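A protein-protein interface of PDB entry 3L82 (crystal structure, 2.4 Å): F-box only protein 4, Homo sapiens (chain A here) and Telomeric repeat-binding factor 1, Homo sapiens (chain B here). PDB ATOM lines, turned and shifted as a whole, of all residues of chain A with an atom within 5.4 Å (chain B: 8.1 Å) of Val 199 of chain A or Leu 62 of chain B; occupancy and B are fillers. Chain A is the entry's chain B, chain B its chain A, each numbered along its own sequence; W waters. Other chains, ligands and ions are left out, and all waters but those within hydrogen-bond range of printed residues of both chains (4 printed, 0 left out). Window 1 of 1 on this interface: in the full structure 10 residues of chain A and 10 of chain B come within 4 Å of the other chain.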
ATOM      1  N   LEU A 166     -13.411 -12.217  -0.469  1.00  0.00           N
ATOM      2  CA  LEU A 166     -12.380 -13.228  -0.264  1.00  0.00           C
ATOM      3  C   LEU A 166     -12.959 -14.336   0.604  1.00  0.00           C
ATOM      4  O   LEU A 166     -13.489 -14.070   1.691  1.00  0.00           O
ATOM      5  CB  LEU A 166     -11.145 -12.614   0.412  1.00  0.00           C
ATOM      6  CG  LEU A 166     -10.041 -13.605   0.810  1.00  0.00           C
ATOM      7  CD1 LEU A 166      -9.438 -14.225  -0.444  1.00  0.00           C
ATOM      8  CD2 LEU A 166      -8.964 -12.901   1.623  1.00  0.00           C
ATOM      9  N   VAL A 167     -12.890 -15.572   0.108  1.00  0.00           N
ATOM     10  CA  VAL A 167     -13.384 -16.728   0.857  1.00  0.00           C
ATOM     11  C   VAL A 167     -12.192 -17.518   1.383  1.00  0.00           C
ATOM     12  O   VAL A 167     -11.353 -17.983   0.613  1.00  0.00           O
ATOM     13  CB  VAL A 167     -14.231 -17.703  -0.014  1.00  0.00           C
ATOM     14  CG1 VAL A 167     -14.676 -18.894   0.835  1.00  0.00           C
ATOM     15  CG2 VAL A 167     -15.444 -17.000  -0.575  1.00  0.00           C
ATOM     16  N   SER A 169     -11.011 -20.840   2.986  1.00  0.00           N
ATOM     17  CA  SER A 169     -11.393 -22.241   3.204  1.00  0.00           C
ATOM     18  C   SER A 169     -10.433 -22.636   4.295  1.00  0.00           C
ATOM     19  O   SER A 169      -9.267 -22.937   4.026  1.00  0.00           O
ATOM     20  CB  SER A 169     -11.124 -23.089   1.956  1.00  0.00           C
ATOM     21  OG  SER A 169     -12.044 -22.771   0.943  1.00  0.00           O
ATOM     22  N   CYS A 181     -11.094 -26.933  -2.483  1.00  0.00           N
ATOM     23  CA  CYS A 181     -11.702 -25.633  -2.743  1.00  0.00           C
ATOM     24  C   CYS A 181     -12.687 -25.569  -3.918  1.00  0.00           C
ATOM     25  O   CYS A 181     -13.611 -24.742  -3.914  1.00  0.00           O
ATOM     26  CB  CYS A 181     -10.613 -24.561  -2.885  1.00  0.00           C
ATOM     27  SG  CYS A 181      -9.399 -24.826  -4.195  1.00  0.00           S
ATOM     28  N   PHE A 182     -12.512 -26.429  -4.916  1.00  0.00           N
ATOM     29  CA  PHE A 182     -13.445 -26.432  -6.038  1.00  0.00           C
ATOM     30  C   PHE A 182     -14.851 -26.759  -5.543  1.00  0.00           C
ATOM     31  O   PHE A 182     -15.828 -26.087  -5.877  1.00  0.00           O
ATOM     32  CB  PHE A 182     -13.057 -27.478  -7.081  1.00  0.00           C
ATOM     33  CG  PHE A 182     -14.202 -27.889  -7.970  1.00  0.00           C
ATOM     34  CD1 PHE A 182     -14.752 -29.161  -7.873  1.00  0.00           C
ATOM     35  CD2 PHE A 182     -14.743 -26.997  -8.891  1.00  0.00           C
ATOM     36  CE1 PHE A 182     -15.828 -29.544  -8.687  1.00  0.00           C
ATOM     37  CE2 PHE A 182     -15.816 -27.363  -9.708  1.00  0.00           C
ATOM     38  CZ  PHE A 182     -16.362 -28.641  -9.610  1.00  0.00           C
ATOM     39  N   LEU A 184     -16.180 -26.293  -2.763  1.00  0.00           N
ATOM     40  CA  LEU A 184     -16.719 -25.177  -1.986  1.00  0.00           C
ATOM     41  C   LEU A 184     -17.291 -24.068  -2.871  1.00  0.00           C
ATOM     42  O   LEU A 184     -18.403 -23.587  -2.636  1.00  0.00           O
ATOM     43  CB  LEU A 184     -15.619 -24.622  -1.084  1.00  0.00           C
ATOM     44  CG  LEU A 184     -16.072 -23.985   0.221  1.00  0.00           C
ATOM     45  CD1 LEU A 184     -14.924 -24.020   1.225  1.00  0.00           C
ATOM     46  CD2 LEU A 184     -16.539 -22.570  -0.039  1.00  0.00           C
ATOM     47  N   ALA A 185     -16.538 -23.661  -3.889  1.00  0.00           N
ATOM     48  CA  ALA A 185     -17.013 -22.619  -4.795  1.00  0.00           C
ATOM     49  C   ALA A 185     -18.275 -23.103  -5.493  1.00  0.00           C
ATOM     50  O   ALA A 185     -19.220 -22.337  -5.696  1.00  0.00           O
ATOM     51  CB  ALA A 185     -15.944 -22.279  -5.826  1.00  0.00           C
ATOM     52  N   LEU A 190     -21.060 -19.092  -5.987  1.00  0.00           N
ATOM     53  CA  LEU A 190     -20.491 -17.757  -5.872  1.00  0.00           C
ATOM     54  C   LEU A 190     -20.799 -16.806  -7.040  1.00  0.00           C
ATOM     55  O   LEU A 190     -20.728 -15.581  -6.880  1.00  0.00           O
ATOM     56  CB  LEU A 190     -18.970 -17.856  -5.659  1.00  0.00           C
ATOM     57  CG  LEU A 190     -18.528 -18.584  -4.381  1.00  0.00           C
ATOM     58  CD1 LEU A 190     -17.002 -18.743  -4.357  1.00  0.00           C
ATOM     59  CD2 LEU A 190     -19.019 -17.813  -3.164  1.00  0.00           C
ATOM     60  N   TRP A 197     -14.641 -12.647  -7.016  1.00  0.00           N
ATOM     61  CA  TRP A 197     -14.229 -13.449  -5.870  1.00  0.00           C
ATOM     62  C   TRP A 197     -12.960 -14.279  -5.979  1.00  0.00           C
ATOM     63  O   TRP A 197     -12.348 -14.382  -7.036  1.00  0.00           O
ATOM     64  CB  TRP A 197     -15.371 -14.379  -5.477  1.00  0.00           C
ATOM     65  CG  TRP A 197     -15.841 -15.311  -6.585  1.00  0.00           C
ATOM     66  CD1 TRP A 197     -16.897 -15.112  -7.434  1.00  0.00           C
ATOM     67  CD2 TRP A 197     -15.307 -16.601  -6.911  1.00  0.00           C
ATOM     68  NE1 TRP A 197     -17.057 -16.198  -8.258  1.00  0.00           N
ATOM     69  CE2 TRP A 197     -16.095 -17.127  -7.962  1.00  0.00           C
ATOM     70  CE3 TRP A 197     -14.239 -17.366  -6.418  1.00  0.00           C
ATOM     71  CZ2 TRP A 197     -15.852 -18.389  -8.528  1.00  0.00           C
ATOM     72  CZ3 TRP A 197     -13.997 -18.624  -6.982  1.00  0.00           C
ATOM     73  CH2 TRP A 197     -14.802 -19.120  -8.025  1.00  0.00           C
ATOM     74  N   LEU A 198     -12.572 -14.868  -4.853  1.00  0.00           N
ATOM     75  CA  LEU A 198     -11.409 -15.743  -4.797  1.00  0.00           C
ATOM     76  C   LEU A 198     -11.495 -16.673  -3.586  1.00  0.00           C
ATOM     77  O   LEU A 198     -11.881 -16.249  -2.499  1.00  0.00           O
ATOM     78  CB  LEU A 198     -10.114 -14.940  -4.711  1.00  0.00           C
ATOM     79  CG  LEU A 198      -8.924 -15.832  -4.330  1.00  0.00           C
ATOM     80  CD1 LEU A 198      -8.567 -16.726  -5.507  1.00  0.00           C
ATOM     81  CD2 LEU A 198      -7.725 -14.998  -3.929  1.00  0.00           C
ATOM     82  N   VAL A 199     -11.166 -17.950  -3.783  1.00  0.00           N
ATOM     83  CA  VAL A 199     -11.171 -18.901  -2.684  1.00  0.00           C
ATOM     84  C   VAL A 199      -9.720 -19.275  -2.439  1.00  0.00           C
ATOM     85  O   VAL A 199      -9.017 -19.651  -3.368  1.00  0.00           O
ATOM     86  CB  VAL A 199     -11.951 -20.177  -2.999  1.00  0.00           C
ATOM     87  CG1 VAL A 199     -12.027 -21.045  -1.732  1.00  0.00           C
ATOM     88  CG2 VAL A 199     -13.347 -19.837  -3.507  1.00  0.00           C
ATOM     89  N   GLN A 200      -9.284 -19.159  -1.183  1.00  0.00           N
ATOM     90  CA  GLN A 200      -7.906 -19.453  -0.794  1.00  0.00           C
ATOM     91  C   GLN A 200      -7.865 -20.396   0.421  1.00  0.00           C
ATOM     92  O   GLN A 200      -8.599 -20.191   1.389  1.00  0.00           O
ATOM     93  CB  GLN A 200      -7.187 -18.122  -0.485  1.00  0.00           C
ATOM     94  CG  GLN A 200      -5.855 -18.239   0.240  1.00  0.00           C
ATOM     95  CD  GLN A 200      -4.759 -18.779  -0.638  1.00  0.00           C
ATOM     96  OE1 GLN A 200      -4.390 -18.164  -1.633  1.00  0.00           O
ATOM     97  NE2 GLN A 200      -4.231 -19.939  -0.278  1.00  0.00           N
ATOM     98  N   ASP A 201      -7.026 -21.433   0.356  1.00  0.00           N
ATOM     99  CA  ASP A 201      -6.898 -22.399   1.453  1.00  0.00           C
ATOM    100  C   ASP A 201      -6.123 -21.795   2.617  1.00  0.00           C
ATOM    101  O   ASP A 201      -5.074 -21.180   2.416  1.00  0.00           O
ATOM    102  CB  ASP A 201      -6.178 -23.676   0.985  1.00  0.00           C
ATOM    103  CG  ASP A 201      -7.093 -24.631   0.193  1.00  0.00           C
ATOM    104  OD1 ASP A 201      -8.264 -24.274  -0.087  1.00  0.00           O
ATOM    105  OD2 ASP A 201      -6.629 -25.745  -0.154  1.00  0.00           O
ATOM    106  N   ALA B  19       0.963 -22.169  -7.487  1.00  0.00           N
ATOM    107  CA  ALA B  19      -0.389 -21.833  -7.915  1.00  0.00           C
ATOM    108  C   ALA B  19      -0.361 -21.445  -9.391  1.00  0.00           C
ATOM    109  O   ALA B  19      -1.262 -21.810 -10.152  1.00  0.00           O
ATOM    110  CB  ALA B  19      -0.948 -20.680  -7.075  1.00  0.00           C
ATOM    111  N   LEU B  26      -3.719 -26.802 -15.671  1.00  0.00           N
ATOM    112  CA  LEU B  26      -5.164 -26.946 -15.804  1.00  0.00           C
ATOM    113  C   LEU B  26      -5.657 -26.582 -17.208  1.00  0.00           C
ATOM    114  O   LEU B  26      -6.435 -27.326 -17.804  1.00  0.00           O
ATOM    115  CB  LEU B  26      -5.884 -26.093 -14.755  1.00  0.00           C
ATOM    116  CG  LEU B  26      -7.416 -26.174 -14.725  1.00  0.00           C
ATOM    117  CD1 LEU B  26      -7.895 -27.617 -14.530  1.00  0.00           C
ATOM    118  CD2 LEU B  26      -7.923 -25.300 -13.604  1.00  0.00           C
ATOM    119  N   ILE B  56      -7.068 -31.028 -10.086  1.00  0.00           N
ATOM    120  CA  ILE B  56      -8.130 -30.226  -9.475  1.00  0.00           C
ATOM    121  C   ILE B  56      -8.142 -30.419  -7.951  1.00  0.00           C
ATOM    122  O   ILE B  56      -8.353 -29.469  -7.199  1.00  0.00           O
ATOM    123  CB  ILE B  56      -9.519 -30.604 -10.037  1.00  0.00           C
ATOM    124  CG1 ILE B  56      -9.566 -30.319 -11.540  1.00  0.00           C
ATOM    125  CG2 ILE B  56     -10.612 -29.806  -9.337  1.00  0.00           C
ATOM    126  CD1 ILE B  56     -10.852 -30.800 -12.199  1.00  0.00           C
ATOM    127  N   LEU B  59      -5.396 -28.205  -6.096  1.00  0.00           N
ATOM    128  CA  LEU B  59      -5.416 -26.744  -6.147  1.00  0.00           C
ATOM    129  C   LEU B  59      -5.546 -26.107  -4.760  1.00  0.00           C
ATOM    130  O   LEU B  59      -6.326 -26.566  -3.931  1.00  0.00           O
ATOM    131  CB  LEU B  59      -6.577 -26.264  -7.022  1.00  0.00           C
ATOM    132  CG  LEU B  59      -6.532 -26.570  -8.517  1.00  0.00           C
ATOM    133  CD1 LEU B  59      -7.840 -26.135  -9.168  1.00  0.00           C
ATOM    134  CD2 LEU B  59      -5.356 -25.839  -9.149  1.00  0.00           C
ATOM    135  N   SER B  60      -4.795 -25.038  -4.520  1.00  0.00           N
ATOM    136  CA  SER B  60      -4.851 -24.346  -3.237  1.00  0.00           C
ATOM    137  C   SER B  60      -5.660 -23.043  -3.296  1.00  0.00           C
ATOM    138  O   SER B  60      -5.918 -22.422  -2.262  1.00  0.00           O
ATOM    139  CB  SER B  60      -3.431 -24.062  -2.732  1.00  0.00           C
ATOM    140  OG  SER B  60      -2.741 -25.279  -2.500  1.00  0.00           O
ATOM    141  N   SER B  61      -6.051 -22.631  -4.500  1.00  0.00           N
ATOM    142  CA  SER B  61      -6.847 -21.416  -4.683  1.00  0.00           C
ATOM    143  C   SER B  61      -7.687 -21.540  -5.945  1.00  0.00           C
ATOM    144  O   SER B  61      -7.445 -22.428  -6.764  1.00  0.00           O
ATOM    145  CB  SER B  61      -5.948 -20.182  -4.768  1.00  0.00           C
ATOM    146  OG  SER B  61      -4.949 -20.356  -5.756  1.00  0.00           O
ATOM    147  N   LEU B  62      -8.660 -20.649  -6.118  1.00  0.00           N
ATOM    148  CA  LEU B  62      -9.542 -20.745  -7.272  1.00  0.00           C
ATOM    149  C   LEU B  62     -10.203 -19.418  -7.653  1.00  0.00           C
ATOM    150  O   LEU B  62     -10.575 -18.647  -6.778  1.00  0.00           O
ATOM    151  CB  LEU B  62     -10.637 -21.767  -6.954  1.00  0.00           C
ATOM    152  CG  LEU B  62     -11.190 -22.728  -8.004  1.00  0.00           C
ATOM    153  CD1 LEU B  62     -12.687 -22.824  -7.798  1.00  0.00           C
ATOM    154  CD2 LEU B  62     -10.883 -22.257  -9.405  1.00  0.00           C
ATOM    155  N   THR B  63     -10.358 -19.176  -8.957  1.00  0.00           N
ATOM    156  CA  THR B  63     -11.023 -17.968  -9.480  1.00  0.00           C
ATOM    157  C   THR B  63     -12.197 -18.420 -10.369  1.00  0.00           C
ATOM    158  O   THR B  63     -12.331 -19.607 -10.668  1.00  0.00           O
ATOM    159  CB  THR B  63     -10.093 -17.151 -10.372  1.00  0.00           C
ATOM    160  OG1 THR B  63     -10.020 -17.781 -11.656  1.00  0.00           O
ATOM    161  CG2 THR B  63      -8.685 -17.086  -9.775  1.00  0.00           C
ATOM    162  N   ALA B  64     -13.038 -17.479 -10.797  1.00  0.00           N
ATOM    163  CA  ALA B  64     -14.189 -17.786 -11.659  1.00  0.00           C
ATOM    164  C   ALA B  64     -13.760 -18.352 -13.023  1.00  0.00           C
ATOM    165  O   ALA B  64     -14.465 -19.171 -13.628  1.00  0.00           O
ATOM    166  CB  ALA B  64     -15.030 -16.535 -11.868  1.00  0.00           C
ATOM    167  N   CYS B  65     -12.598 -17.909 -13.492  1.00  0.00           N
ATOM    168  CA  CYS B  65     -12.047 -18.348 -14.766  1.00  0.00           C
ATOM    169  C   CYS B  65     -11.638 -19.813 -14.717  1.00  0.00           C
ATOM    170  O   CYS B  65     -11.890 -20.582 -15.655  1.00  0.00           O
ATOM    171  CB  CYS B  65     -10.826 -17.490 -15.127  1.00  0.00           C
ATOM    172  SG  CYS B  65      -9.749 -18.195 -16.411  1.00  0.00           S
ATOM    173  N   GLN B  66     -10.984 -20.198 -13.629  1.00  0.00           N
ATOM    174  CA  GLN B  66     -10.545 -21.578 -13.475  1.00  0.00           C
ATOM    175  C   GLN B  66     -11.756 -22.471 -13.215  1.00  0.00           C
ATOM    176  O   GLN B  66     -11.799 -23.603 -13.672  1.00  0.00           O
ATOM    177  CB  GLN B  66      -9.549 -21.682 -12.327  1.00  0.00           C
ATOM    178  CG  GLN B  66      -8.290 -20.861 -12.538  1.00  0.00           C
ATOM    179  CD  GLN B  66      -7.441 -20.815 -11.278  1.00  0.00           C
ATOM    180  OE1 GLN B  66      -7.908 -20.381 -10.219  1.00  0.00           O
ATOM    181  NE2 GLN B  66      -6.191 -21.267 -11.383  1.00  0.00           N
ATOM    182  N   LEU B  67     -12.741 -21.951 -12.490  1.00  0.00           N
ATOM    183  CA  LEU B  67     -13.949 -22.721 -12.217  1.00  0.00           C
ATOM    184  C   LEU B  67     -14.690 -23.054 -13.517  1.00  0.00           C
ATOM    185  O   LEU B  67     -15.200 -24.166 -13.679  1.00  0.00           O
ATOM    186  CB  LEU B  67     -14.901 -21.957 -11.287  1.00  0.00           C
ATOM    187  CG  LEU B  67     -16.202 -22.730 -11.010  1.00  0.00           C
ATOM    188  CD1 LEU B  67     -15.846 -24.052 -10.325  1.00  0.00           C
ATOM    189  CD2 LEU B  67     -17.153 -21.923 -10.139  1.00  0.00           C
ATOM    190  N   ARG B  68     -14.746 -22.095 -14.441  1.00  0.00           N
ATOM    191  CA  ARG B  68     -15.438 -22.307 -15.719  1.00  0.00           C
ATOM    192  C   ARG B  68     -14.718 -23.384 -16.532  1.00  0.00           C
ATOM    193  O   ARG B  68     -15.357 -24.240 -17.152  1.00  0.00           O
ATOM    194  CB  ARG B  68     -15.519 -20.989 -16.505  1.00  0.00           C
ATOM    195  CG  ARG B  68     -16.230 -21.081 -17.851  1.00  0.00           C
ATOM    196  CD  ARG B  68     -16.583 -19.692 -18.389  1.00  0.00           C
ATOM    197  NE  ARG B  68     -16.939 -19.737 -19.805  1.00  0.00           N
ATOM    198  CZ  ARG B  68     -16.054 -19.848 -20.795  1.00  0.00           C
ATOM    199  NH1 ARG B  68     -14.752 -19.913 -20.533  1.00  0.00           N
ATOM    200  NH2 ARG B  68     -16.476 -19.928 -22.051  1.00  0.00           N
ATOM    201  N   THR B  69     -13.387 -23.346 -16.505  1.00  0.00           N
ATOM    202  CA  THR B  69     -12.574 -24.335 -17.199  1.00  0.00           C
ATOM    203  C   THR B  69     -12.871 -25.728 -16.625  1.00  0.00           C
ATOM    204  O   THR B  69     -12.905 -26.719 -17.358  1.00  0.00           O
ATOM    205  CB  THR B  69     -11.080 -24.033 -17.021  1.00  0.00           C
ATOM    206  OG1 THR B  69     -10.807 -22.722 -17.523  1.00  0.00           O
ATOM    207  CG2 THR B  69     -10.220 -25.052 -17.759  1.00  0.00           C
ATOM    208  N   ILE B  70     -13.087 -25.808 -15.314  1.00  0.00           N
ATOM    209  CA  ILE B  70     -13.384 -27.096 -14.696  1.00  0.00           C
ATOM    210  C   ILE B  70     -14.759 -27.598 -15.145  1.00  0.00           C
ATOM    211  O   ILE B  70     -14.917 -28.764 -15.494  1.00  0.00           O
ATOM    212  CB  ILE B  70     -13.307 -26.996 -13.153  1.00  0.00           C
ATOM    213  CG1 ILE B  70     -11.841 -26.769 -12.743  1.00  0.00           C
ATOM    214  CG2 ILE B  70     -13.877 -28.268 -12.506  1.00  0.00           C
ATOM    215  CD1 ILE B  70     -11.614 -26.607 -11.264  1.00  0.00           C
HETATM  216  O   HOH W   1     -12.845 -14.372 -10.056  1.00  0.00           O
HETATM  217  O   HOH W   2      -9.807 -27.944  -5.325  1.00  0.00           O
HETATM  218  O   HOH W   3      -8.241 -27.612  -2.231  1.00  0.00           O
HETATM  219  O   HOH W   4      -4.113 -26.866   0.121  1.00  0.00           O
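Water W3 lies within hydrogen-bond range of the backbone carbonyl oxygen of Leu 59 of chain B, the backbone NH of Cys 181 of chain A and the side-chain carboxylate of Asp 201 of chain A. Water W4 lies within hydrogen-bond range of OD2 of Asp 201 of chain A (2.8 Å) and OG of Ser 60 of chain B (3.4 Å). Water W2 lies within hydrogen-bond range of the backbone carbonyl oxygen (O) of Ile 56 of chain B, the backbone NH (N) of Phe 182 of chain A and the backbone NH (N) of Cys 181 of chain A. Water W1 bridges O of Trp 197 of chain A (3.1 Å) and N of Ala 64 of chain B (3.2 Å).
Leu 67 of chain B touches Phe 182 of chain A (CD1 to CE2, 3.4 Å). Phe 182 of chain A touches Ile 70 of chain B. CB of Ala 185 of chain A touches CD1 of Leu 62 of chain B, 3.8 Å away. O of Leu 62 of chain B touches CZ3 of Trp 197 of chain A (3.4 Å). Thr 63 of chain B touches Trp 197 of chain A. Trp 197 of chain A touches Ala 64 of chain B. Leu 62 of chain B touches Leu 198 of chain A. Ser 61 of chain B touches Val 199 of chain A (CA to O, 3.1 Å). NE2 of Gln 200 of chain A touches O of Ser 60 of chain B, 3.6 Å away. Asp 201 of chain A touches Leu 59 of chain B.
SG of Cys 181 of chain A lies within hydrogen-bond range of O of Leu 59 of chain B (3.5 Å). O of Ser 60 of chain B sits at hydrogen-bond distance from N of Asp 201 of chain A, 3.0 Å away. O of Val 199 of chain A lies within hydrogen-bond range of N of Leu 62 of chain B (2.9 Å).
Val 167 of chain A touches none of the printed residues of chain B. Of the printed residues of chain B, Cys 181 of chain A touches Leu 59. Printed residues of chain B within 4 Å of Val 199 of chain A: Ser 61 (3.1 Å) and Leu 62 (2.9 Å). Of the printed residues of chain B, Gln 200 of chain A touches Ser 60. Of the printed residues of chain A, Leu 62 of chain B touches Ala 185 (3.8 Å), Trp 197 (3.4 Å), Leu 198 (3.1 Å) and Val 199 (2.9 Å). The nearest residue of chain B that does not touch Val 199 of chain A is Ser 60 of chain B (4.3 Å). The nearest printed residue of chain B that does not touch Gln 200 of chain A is Ser 61 of chain B (4.04 Å).
Hydrophobic or aromatic side chains of chain A that line the printed part of chain B: Phe 182, Ala 185, Trp 197 and Leu 198. Among the printed residues, 13 pairs touch across the chains. Among the printed residues, no Asp or Glu carboxylate lies within 4 Å of a Lys or Arg side-chain nitrogen of the other chain.
OG1 of Thr 63 of chain B sits at hydrogen-bond distance from N of Cys 65 of chain B (3.2 Å). The backbone NH (N) of Thr 63 of chain B is in hydrogen-bond range of the side-chain amide oxygen (OE1) of Gln 66 of chain B. O of Leu 198 of chain A sits at hydrogen-bond distance from N of Val 167 of chain A. The backbone carbonyl oxygen of Val 167 of chain A sits at hydrogen-bond distance from the backbone NH of Gln 200 of chain A, 3.0 Å away. The backbone NH (N) of Ser 169 of chain A is in hydrogen-bond range of the backbone carbonyl oxygen (O) of Gln 200 of chain A.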
